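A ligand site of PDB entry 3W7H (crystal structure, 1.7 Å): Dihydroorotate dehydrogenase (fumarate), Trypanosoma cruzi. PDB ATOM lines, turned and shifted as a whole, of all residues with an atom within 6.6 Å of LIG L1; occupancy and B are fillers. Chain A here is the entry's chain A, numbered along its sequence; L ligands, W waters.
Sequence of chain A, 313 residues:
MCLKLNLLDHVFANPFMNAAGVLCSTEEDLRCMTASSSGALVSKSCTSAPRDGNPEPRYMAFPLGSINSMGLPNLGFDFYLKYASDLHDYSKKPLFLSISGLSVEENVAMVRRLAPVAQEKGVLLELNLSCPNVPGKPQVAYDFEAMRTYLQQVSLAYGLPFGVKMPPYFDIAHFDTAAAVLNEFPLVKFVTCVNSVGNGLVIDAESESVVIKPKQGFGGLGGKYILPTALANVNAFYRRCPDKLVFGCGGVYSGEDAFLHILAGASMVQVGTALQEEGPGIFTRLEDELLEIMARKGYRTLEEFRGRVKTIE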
ATOM      1  N   ALA A  20      14.469  -5.927   7.037  1.00  0.00           N
ATOM      2  CA  ALA A  20      14.955  -6.548   8.180  1.00  0.00           C
ATOM      3  C   ALA A  20      14.677  -5.701   9.426  1.00  0.00           C
ATOM      4  O   ALA A  20      14.742  -4.480   9.387  1.00  0.00           O
ATOM      5  CB  ALA A  20      16.511  -6.807   8.089  1.00  0.00           C
ATOM      6  N   LYS A  44      15.139 -10.961  11.394  1.00  0.00           N
ATOM      7  CA  LYS A  44      15.780  -9.956  12.147  1.00  0.00           C
ATOM      8  C   LYS A  44      17.266 -10.174  12.154  1.00  0.00           C
ATOM      9  O   LYS A  44      17.725 -11.262  12.446  1.00  0.00           O
ATOM     10  CB  LYS A  44      15.279 -10.003  13.528  1.00  0.00           C
ATOM     11  CG  LYS A  44      15.966  -9.091  14.491  1.00  0.00           C
ATOM     12  CD  LYS A  44      15.868  -7.604  14.274  1.00  0.00           C
ATOM     13  CE  LYS A  44      16.886  -6.771  15.057  1.00  0.00           C
ATOM     14  NZ  LYS A  44      16.732  -5.243  14.858  1.00  0.00           N
ATOM     15  N   SER A  45      18.028  -9.097  11.913  1.00  0.00           N
ATOM     16  CA  SER A  45      19.501  -9.118  11.970  1.00  0.00           C
ATOM     17  C   SER A  45      19.868  -9.728  13.305  1.00  0.00           C
ATOM     18  O   SER A  45      19.372  -9.321  14.328  1.00  0.00           O
ATOM     19  CB  SER A  45      20.082  -7.781  11.877  1.00  0.00           C
ATOM     20  OG  SER A  45      19.975  -7.319  10.559  1.00  0.00           O
ATOM     21  N   ARG A  51      20.063 -10.926  22.387  1.00  0.00           N
ATOM     22  CA  ARG A  51      20.137  -9.596  22.904  1.00  0.00           C
ATOM     23  C   ARG A  51      18.752  -9.069  23.234  1.00  0.00           C
ATOM     24  O   ARG A  51      17.821  -9.296  22.531  1.00  0.00           O
ATOM     25  CB  ARG A  51      20.697  -8.637  21.896  1.00  0.00           C
ATOM     26  CG  ARG A  51      22.157  -8.831  21.666  1.00  0.00           C
ATOM     27  CD  ARG A  51      22.639  -7.958  20.546  1.00  0.00           C
ATOM     28  NE  ARG A  51      22.448  -6.544  20.757  1.00  0.00           N
ATOM     29  CZ  ARG A  51      23.323  -5.780  21.358  1.00  0.00           C
ATOM     30  NH1 ARG A  51      24.446  -6.312  21.794  1.00  0.00           N
ATOM     31  NH2 ARG A  51      23.063  -4.500  21.511  1.00  0.00           N
ATOM     32  N   ASN A  54      18.036  -2.180  23.356  1.00  0.00           N
ATOM     33  CA  ASN A  54      18.057  -0.979  24.141  1.00  0.00           C
ATOM     34  C   ASN A  54      16.787  -0.733  24.965  1.00  0.00           C
ATOM     35  O   ASN A  54      15.752  -1.358  24.736  1.00  0.00           O
ATOM     36  CB  ASN A  54      18.190   0.183  23.174  1.00  0.00           C
ATOM     37  CG  ASN A  54      19.572   0.380  22.665  1.00  0.00           C
ATOM     38  OD1 ASN A  54      20.563  -0.174  23.235  1.00  0.00           O
ATOM     39  ND2 ASN A  54      19.697   1.037  21.538  1.00  0.00           N
ATOM     40  N   ASN A  68      14.222   4.984  15.207  1.00  0.00           N
ATOM     41  CA  ASN A  68      14.477   3.887  16.092  1.00  0.00           C
ATOM     42  C   ASN A  68      15.901   3.812  16.559  1.00  0.00           C
ATOM     43  O   ASN A  68      16.848   4.134  15.804  1.00  0.00           O
ATOM     44  CB  ASN A  68      14.076   2.555  15.432  1.00  0.00           C
ATOM     45  CG  ASN A  68      15.197   1.981  14.572  1.00  0.00           C
ATOM     46  OD1 ASN A  68      16.105   1.274  15.118  1.00  0.00           O
ATOM     47  ND2 ASN A  68      15.122   2.138  13.295  1.00  0.00           N
ATOM     48  N   SER A  69      16.090   3.319  17.763  1.00  0.00           N
ATOM     49  CA  SER A  69      17.375   2.855  18.193  1.00  0.00           C
ATOM     50  C   SER A  69      17.093   1.579  18.973  1.00  0.00           C
ATOM     51  O   SER A  69      17.243   1.508  20.196  1.00  0.00           O
ATOM     52  CB  SER A  69      18.142   3.904  19.003  1.00  0.00           C
ATOM     53  OG  SER A  69      19.408   3.338  19.297  1.00  0.00           O
ATOM     54  N   MET A  70      16.770   0.540  18.233  1.00  0.00           N
ATOM     55  CA  MET A  70      16.349  -0.701  18.836  1.00  0.00           C
ATOM     56  C   MET A  70      17.546  -1.387  19.555  1.00  0.00           C
ATOM     57  O   MET A  70      17.362  -1.995  20.598  1.00  0.00           O
ATOM     58  CB  MET A  70      15.857  -1.618  17.804  1.00  0.00           C
ATOM     59  CG  MET A  70      14.737  -1.220  16.905  1.00  0.00           C
ATOM     60  SD  MET A  70      13.276  -0.809  17.805  1.00  0.00           S
ATOM     61  CE  MET A  70      12.639  -2.302  18.338  1.00  0.00           C
ATOM     62  N   GLY A  71      18.768  -1.248  19.035  1.00  0.00           N
ATOM     63  CA  GLY A  71      19.894  -1.893  19.685  1.00  0.00           C
ATOM     64  C   GLY A  71      20.047  -3.385  19.397  1.00  0.00           C
ATOM     65  O   GLY A  71      20.552  -4.108  20.266  1.00  0.00           O
ATOM     66  N   LEU A  72      19.545  -3.867  18.266  1.00  0.00           N
ATOM     67  CA  LEU A  72      19.667  -5.215  17.813  1.00  0.00           C
ATOM     68  C   LEU A  72      19.103  -6.207  18.800  1.00  0.00           C
ATOM     69  O   LEU A  72      19.672  -7.306  19.088  1.00  0.00           O
ATOM     70  CB  LEU A  72      21.167  -5.518  17.485  1.00  0.00           C
ATOM     71  CG  LEU A  72      21.621  -6.367  16.359  1.00  0.00           C
ATOM     72  CD1 LEU A  72      20.814  -6.306  15.070  1.00  0.00           C
ATOM     73  CD2 LEU A  72      23.137  -5.997  16.131  1.00  0.00           C
ATOM     74  N   PRO A  73      17.875  -6.000  19.285  1.00  0.00           N
ATOM     75  CA  PRO A  73      17.219  -7.073  20.042  1.00  0.00           C
ATOM     76  C   PRO A  73      16.964  -8.259  19.126  1.00  0.00           C
ATOM     77  O   PRO A  73      16.488  -8.099  17.994  1.00  0.00           O
ATOM     78  CB  PRO A  73      15.899  -6.481  20.481  1.00  0.00           C
ATOM     79  CG  PRO A  73      15.613  -5.412  19.515  1.00  0.00           C
ATOM     80  CD  PRO A  73      16.906  -4.996  18.809  1.00  0.00           C
ATOM     81  N   SER A 100      24.117  -9.608  11.726  1.00  0.00           N
ATOM     82  CA  SER A 100      24.755  -8.363  12.046  1.00  0.00           C
ATOM     83  C   SER A 100      25.633  -8.503  13.296  1.00  0.00           C
ATOM     84  O   SER A 100      25.440  -7.882  14.377  1.00  0.00           O
ATOM     85  CB  SER A 100      23.640  -7.313  12.218  1.00  0.00           C
ATOM     86  OG  SER A 100      24.184  -6.079  12.554  1.00  0.00           O
ATOM     87  N   LEU A 102      28.783  -8.098  15.733  1.00  0.00           N
ATOM     88  CA  LEU A 102      29.388  -6.912  16.321  1.00  0.00           C
ATOM     89  C   LEU A 102      30.876  -6.799  16.071  1.00  0.00           C
ATOM     90  O   LEU A 102      31.523  -5.811  16.458  1.00  0.00           O
ATOM     91  CB  LEU A 102      29.215  -6.953  17.836  1.00  0.00           C
ATOM     92  CG  LEU A 102      27.764  -7.138  18.342  1.00  0.00           C
ATOM     93  CD1 LEU A 102      27.775  -7.162  19.871  1.00  0.00           C
ATOM     94  CD2 LEU A 102      26.855  -6.103  17.787  1.00  0.00           C
ATOM     95  N   ASN A 128      24.371  -7.375   7.136  1.00  0.00           N
ATOM     96  CA  ASN A 128      24.137  -6.002   7.458  1.00  0.00           C
ATOM     97  C   ASN A 128      25.434  -5.292   7.766  1.00  0.00           C
ATOM     98  O   ASN A 128      26.045  -5.543   8.754  1.00  0.00           O
ATOM     99  CB  ASN A 128      23.253  -5.946   8.694  1.00  0.00           C
ATOM    100  CG  ASN A 128      22.879  -4.545   9.072  1.00  0.00           C
ATOM    101  OD1 ASN A 128      23.156  -3.661   8.439  1.00  0.00           O
ATOM    102  ND2 ASN A 128      22.224  -4.435  10.161  1.00  0.00           N
ATOM    103  N   SER A 130      25.632  -2.137   8.297  1.00  0.00           N
ATOM    104  CA  SER A 130      25.478  -1.179   9.403  1.00  0.00           C
ATOM    105  C   SER A 130      25.804  -1.715  10.778  1.00  0.00           C
ATOM    106  O   SER A 130      25.522  -1.062  11.713  1.00  0.00           O
ATOM    107  CB  SER A 130      24.119  -0.570   9.468  1.00  0.00           C
ATOM    108  OG  SER A 130      23.855   0.183   8.320  1.00  0.00           O
ATOM    109  N   CYS A 131      26.372  -2.920  10.953  1.00  0.00           N
ATOM    110  CA  CYS A 131      26.798  -3.358  12.249  1.00  0.00           C
ATOM    111  C   CYS A 131      27.724  -2.142  12.806  1.00  0.00           C
ATOM    112  O   CYS A 131      28.471  -1.519  12.103  1.00  0.00           O
ATOM    113  CB  CYS A 131      27.489  -4.716  12.156  1.00  0.00           C
ATOM    114  SG  CYS A 131      28.618  -5.015  10.733  1.00  0.00           S
ATOM    115  N   PRO A 132      27.467  -1.688  14.048  1.00  0.00           N
ATOM    116  CA  PRO A 132      28.471  -0.873  14.675  1.00  0.00           C
ATOM    117  C   PRO A 132      29.722  -1.698  14.687  1.00  0.00           C
ATOM    118  O   PRO A 132      29.684  -2.853  14.580  1.00  0.00           O
ATOM    119  CB  PRO A 132      27.936  -0.724  16.091  1.00  0.00           C
ATOM    120  CG  PRO A 132      26.472  -0.561  15.886  1.00  0.00           C
ATOM    121  CD  PRO A 132      26.150  -1.196  14.531  1.00  0.00           C
ATOM    122  N   LYS A 165      23.422  -5.403   3.125  1.00  0.00           N
ATOM    123  CA  LYS A 165      22.512  -4.280   3.442  1.00  0.00           C
ATOM    124  C   LYS A 165      23.371  -3.060   3.743  1.00  0.00           C
ATOM    125  O   LYS A 165      24.258  -3.070   4.600  1.00  0.00           O
ATOM    126  CB  LYS A 165      21.649  -4.641   4.635  1.00  0.00           C
ATOM    127  CG  LYS A 165      20.770  -3.511   5.176  1.00  0.00           C
ATOM    128  CD  LYS A 165      19.485  -3.381   4.336  1.00  0.00           C
ATOM    129  CE  LYS A 165      18.423  -2.560   4.966  1.00  0.00           C
ATOM    130  NZ  LYS A 165      17.751  -3.239   6.025  1.00  0.00           N
ATOM    131  N   ASN A 195      19.506   1.004   4.431  1.00  0.00           N
ATOM    132  CA  ASN A 195      19.162   1.015   5.860  1.00  0.00           C
ATOM    133  C   ASN A 195      18.706   2.424   6.278  1.00  0.00           C
ATOM    134  O   ASN A 195      18.642   3.278   5.495  1.00  0.00           O
ATOM    135  CB  ASN A 195      20.411   0.574   6.691  1.00  0.00           C
ATOM    136  CG  ASN A 195      20.053  -0.169   7.957  1.00  0.00           C
ATOM    137  OD1 ASN A 195      19.285   0.282   8.684  1.00  0.00           O
ATOM    138  ND2 ASN A 195      20.693  -1.285   8.185  1.00  0.00           N
ATOM    139  N   SER A 196      18.394   2.587   7.557  1.00  0.00           N
ATOM    140  CA  SER A 196      17.810   3.830   7.996  1.00  0.00           C
ATOM    141  C   SER A 196      18.803   4.990   7.864  1.00  0.00           C
ATOM    142  O   SER A 196      19.968   4.771   7.801  1.00  0.00           O
ATOM    143  CB  SER A 196      17.339   3.665   9.427  1.00  0.00           C
ATOM    144  OG  SER A 196      18.319   3.165  10.194  1.00  0.00           O
ATOM    145  N   LYS A 215      20.447   6.917  23.320  1.00  0.00           N
ATOM    146  CA  LYS A 215      21.287   7.861  22.545  1.00  0.00           C
ATOM    147  C   LYS A 215      20.735   9.300  22.542  1.00  0.00           C
ATOM    148  O   LYS A 215      20.886  10.056  21.610  1.00  0.00           O
ATOM    149  CB  LYS A 215      21.413   7.347  21.105  1.00  0.00           C
ATOM    150  CG  LYS A 215      22.068   6.003  20.957  1.00  0.00           C
ATOM    151  CD  LYS A 215      22.116   5.571  19.497  1.00  0.00           C
ATOM    152  CE  LYS A 215      22.743   6.611  18.609  1.00  0.00           C
ATOM    153  NZ  LYS A 215      22.942   6.124  17.208  1.00  0.00           N
ATOM    154  N   GLY A 220      17.822   6.006  13.941  1.00  0.00           N
ATOM    155  CA  GLY A 220      17.754   5.945  12.482  1.00  0.00           C
ATOM    156  C   GLY A 220      16.337   6.254  11.983  1.00  0.00           C
ATOM    157  O   GLY A 220      15.351   5.822  12.581  1.00  0.00           O
ATOM    158  N   LEU A 221      16.278   6.968  10.877  1.00  0.00           N
ATOM    159  CA  LEU A 221      15.008   7.408  10.256  1.00  0.00           C
ATOM    160  C   LEU A 221      14.608   6.465   9.137  1.00  0.00           C
ATOM    161  O   LEU A 221      15.427   6.050   8.309  1.00  0.00           O
ATOM    162  CB  LEU A 221      15.177   8.798   9.673  1.00  0.00           C
ATOM    163  CG  LEU A 221      15.628   9.890  10.642  1.00  0.00           C
ATOM    164  CD1 LEU A 221      15.985  11.188   9.851  1.00  0.00           C
ATOM    165  CD2 LEU A 221      14.623  10.108  11.759  1.00  0.00           C
HETATM  166  O1  LIG L   1      18.654  -0.689  16.127  1.00  0.00           O
HETATM  167  C1  LIG L   1      18.662  -1.686  15.390  1.00  0.00           C
HETATM  168  O2  LIG L   1      18.548  -2.838  15.796  1.00  0.00           O
HETATM  169  C2  LIG L   1      18.827  -1.413  13.923  1.00  0.00           C
HETATM  170  N1  LIG L   1      18.009  -0.338  13.477  1.00  0.00           N
HETATM  171  C3  LIG L   1      18.024   0.063  12.174  1.00  0.00           C
HETATM  172  O3  LIG L   1      17.336   1.019  11.815  1.00  0.00           O
HETATM  173  N2  LIG L   1      18.907  -0.598  11.345  1.00  0.00           N
HETATM  174  C4  LIG L   1      19.844  -1.568  11.755  1.00  0.00           C
HETATM  175  O4  LIG L   1      20.579  -2.130  10.930  1.00  0.00           O
HETATM  176  C5  LIG L   1      19.718  -2.021  13.104  1.00  0.00           C
HETATM  177  C6  LIG L   1      20.611  -2.994  13.564  1.00  0.00           C
HETATM  178  C7  LIG L   1      22.112  -2.407  13.671  1.00  0.00           C
HETATM  179  C8  LIG L   1      22.252  -1.677  14.893  1.00  0.00           C
HETATM  180  C9  LIG L   1      22.870  -2.243  16.018  1.00  0.00           C
HETATM  181  C10 LIG L   1      22.937  -1.466  17.234  1.00  0.00           C
HETATM  182  C11 LIG L   1      23.536  -2.009  18.383  1.00  0.00           C
HETATM  183  C12 LIG L   1      23.569  -1.272  19.557  1.00  0.00           C
HETATM  184  C13 LIG L   1      23.072   0.026  19.652  1.00  0.00           C
HETATM  185  C14 LIG L   1      22.528   0.606  18.511  1.00  0.00           C
HETATM  186  C15 LIG L   1      22.429  -0.174  17.323  1.00  0.00           C
HETATM  187  C16 LIG L   1      21.860   0.373  16.181  1.00  0.00           C
HETATM  188  C17 LIG L   1      21.788  -0.361  14.991  1.00  0.00           C
HETATM  189  N1  LG2 L   2      17.823  -3.001   9.149  1.00  0.00           N
HETATM  190  C1  LG2 L   2      18.621  -4.123   9.243  1.00  0.00           C
HETATM  191  O1  LG2 L   2      19.289  -4.393   8.234  1.00  0.00           O
HETATM  192  N2  LG2 L   2      18.603  -4.961  10.297  1.00  0.00           N
HETATM  193  C2  LG2 L   2      17.747  -4.782  11.353  1.00  0.00           C
HETATM  194  O2  LG2 L   2      17.698  -5.574  12.360  1.00  0.00           O
HETATM  195  C3  LG2 L   2      16.918  -3.631  11.367  1.00  0.00           C
HETATM  196  N3  LG2 L   2      16.075  -3.373  12.391  1.00  0.00           N
HETATM  197  C4  LG2 L   2      15.109  -2.370  12.270  1.00  0.00           C
HETATM  198  C5  LG2 L   2      14.113  -2.269  13.269  1.00  0.00           C
HETATM  199  C6  LG2 L   2      13.198  -1.256  13.162  1.00  0.00           C
HETATM  200  C7  LG2 L   2      12.121  -1.084  14.157  1.00  0.00           C
HETATM  201  C8  LG2 L   2      13.191  -0.423  11.970  1.00  0.00           C
HETATM  202  C9  LG2 L   2      12.170   0.610  11.813  1.00  0.00           C
HETATM  203  C10 LG2 L   2      14.161  -0.562  10.980  1.00  0.00           C
HETATM  204  C11 LG2 L   2      15.124  -1.517  11.118  1.00  0.00           C
HETATM  205  N4  LG2 L   2      16.128  -1.697  10.131  1.00  0.00           N
HETATM  206  C12 LG2 L   2      16.966  -2.773  10.164  1.00  0.00           C
HETATM  207  C13 LG2 L   2      16.134  -0.855   8.923  1.00  0.00           C
HETATM  208  C14 LG2 L   2      15.056  -1.273   7.950  1.00  0.00           C
HETATM  209  O3  LG2 L   2      15.393  -2.553   7.464  1.00  0.00           O
HETATM  210  C15 LG2 L   2      15.010  -0.355   6.782  1.00  0.00           C
HETATM  211  O4  LG2 L   2      16.274  -0.389   6.113  1.00  0.00           O
HETATM  212  C16 LG2 L   2      14.696   1.113   7.175  1.00  0.00           C
HETATM  213  O5  LG2 L   2      13.647   1.135   8.177  1.00  0.00           O
HETATM  214  C17 LG2 L   2      14.201   1.910   5.927  1.00  0.00           C
HETATM  215  O6  LG2 L   2      13.041   1.399   5.300  1.00  0.00           O
HETATM  216  P1  LG2 L   2      11.578   2.058   5.569  1.00  0.00           P
HETATM  217  O7  LG2 L   2      10.583   1.194   4.830  1.00  0.00           O
HETATM  218  O8  LG2 L   2      11.671   3.453   5.086  1.00  0.00           O
HETATM  219  O9  LG2 L   2      11.371   1.991   7.076  1.00  0.00           O
HETATM  220  O   HOH W   1      19.137   2.272  15.024  1.00  0.00           O
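Water W1 lies within hydrogen-bond range of O of Asn 68 and O1 of LIG L1.
N of Gly 71 lies within hydrogen-bond range of O1 of LIG L1.
The backbone NH of Met 70 lies within hydrogen-bond range of an oxygen (O1) of LIG L1.
OD1 of Asn 195 lies within hydrogen-bond range of N2 of LIG L1 (2.8 Å).
NZ of Lys 44 is in hydrogen-bond range of O2 of LG2 L2, at 2.7 Å.
OG of Ser 45 lies within hydrogen-bond range of N2 of LG2 L2, 2.7 Å away.
The side-chain amide nitrogen (ND2) of Asn 128 is in hydrogen-bond range of an oxygen (O4) of LIG L1 (2.9 Å).
O of Ala 20 sits at hydrogen-bond distance from O3 of LG2 L2, 2.8 Å away.
The side-chain amide nitrogen (ND2) of Asn 195 lies within hydrogen-bond range of an oxygen (O1) of LG2 L2 (3.4 Å).
The backbone NH of Leu 72 lies within hydrogen-bond range of an oxygen (O2) of LIG L1, 2.9 Å away.
The side-chain amino group (NZ) of Lys 165 lies within hydrogen-bond range of an oxygen (O3) of LG2 L2 (2.8 Å).
O2 of LIG L1 lies within salt-bridge range of NZ of Lys 44 (3.2 Å).
OG of Ser 196 lies within hydrogen-bond range of O3 of LIG L1, at 2.9 Å.
ND2 of Asn 68 lies within hydrogen-bond range of O3 of LIG L1, 2.9 Å away.
O of Asn 128 lies within hydrogen-bond range of SG of Cys 131.
The side-chain amide nitrogen (ND2) of Asn 54 is in hydrogen-bond range of the backbone carbonyl oxygen (O) of Ser 69 (2.8 Å).
The backbone carbonyl oxygen (O) of Asn 68 lies within hydrogen-bond range of the backbone NH (N) of Gly 220 (2.8 Å).
The guanidinium group (NH2) of Arg 51 sits at hydrogen-bond distance from the backbone carbonyl oxygen (O) of Gly 71, 2.8 Å away.
O of Leu 72 lies close to NE of Arg 51 (3.3 Å).
OD1 of Asn 195 is in hydrogen-bond range of OG of Ser 196.
The backbone NH (N) of Asn 54 sits at hydrogen-bond distance from the backbone carbonyl oxygen (O) of Met 70, 2.8 Å away.
The side-chain amide oxygen (OD1) of Asn 68 lies within hydrogen-bond range of the backbone NH (N) of Met 70.
Arg 51 touches LIG L1 (NH2 to C12, 3.8 Å).
Asn 54 touches LIG L1 (ND2 to C13, 3.996 Å).
C of Ser 69 touches O1 of LIG L1, 3.96 Å away.
Pro 132 touches LIG L1.
Within 4 Å of LIG L1: Lys 44, Arg 51, Asn 54, Asn 68, Ser 69, Met 70, Gly 71, Leu 72, Asn 128, Pro 132, Asn 195 and Ser 196.
Along chain A the residues within 4 Å of LIG L1 span positions 44 to 196.
The nearest printed residue that does not touch LIG L1 is Pro 73 (4.1 Å).
A nitrogen (N1) of LG2 L2 sits close to a nitrogen (N2) of LIG L1, at 3.4 Å.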
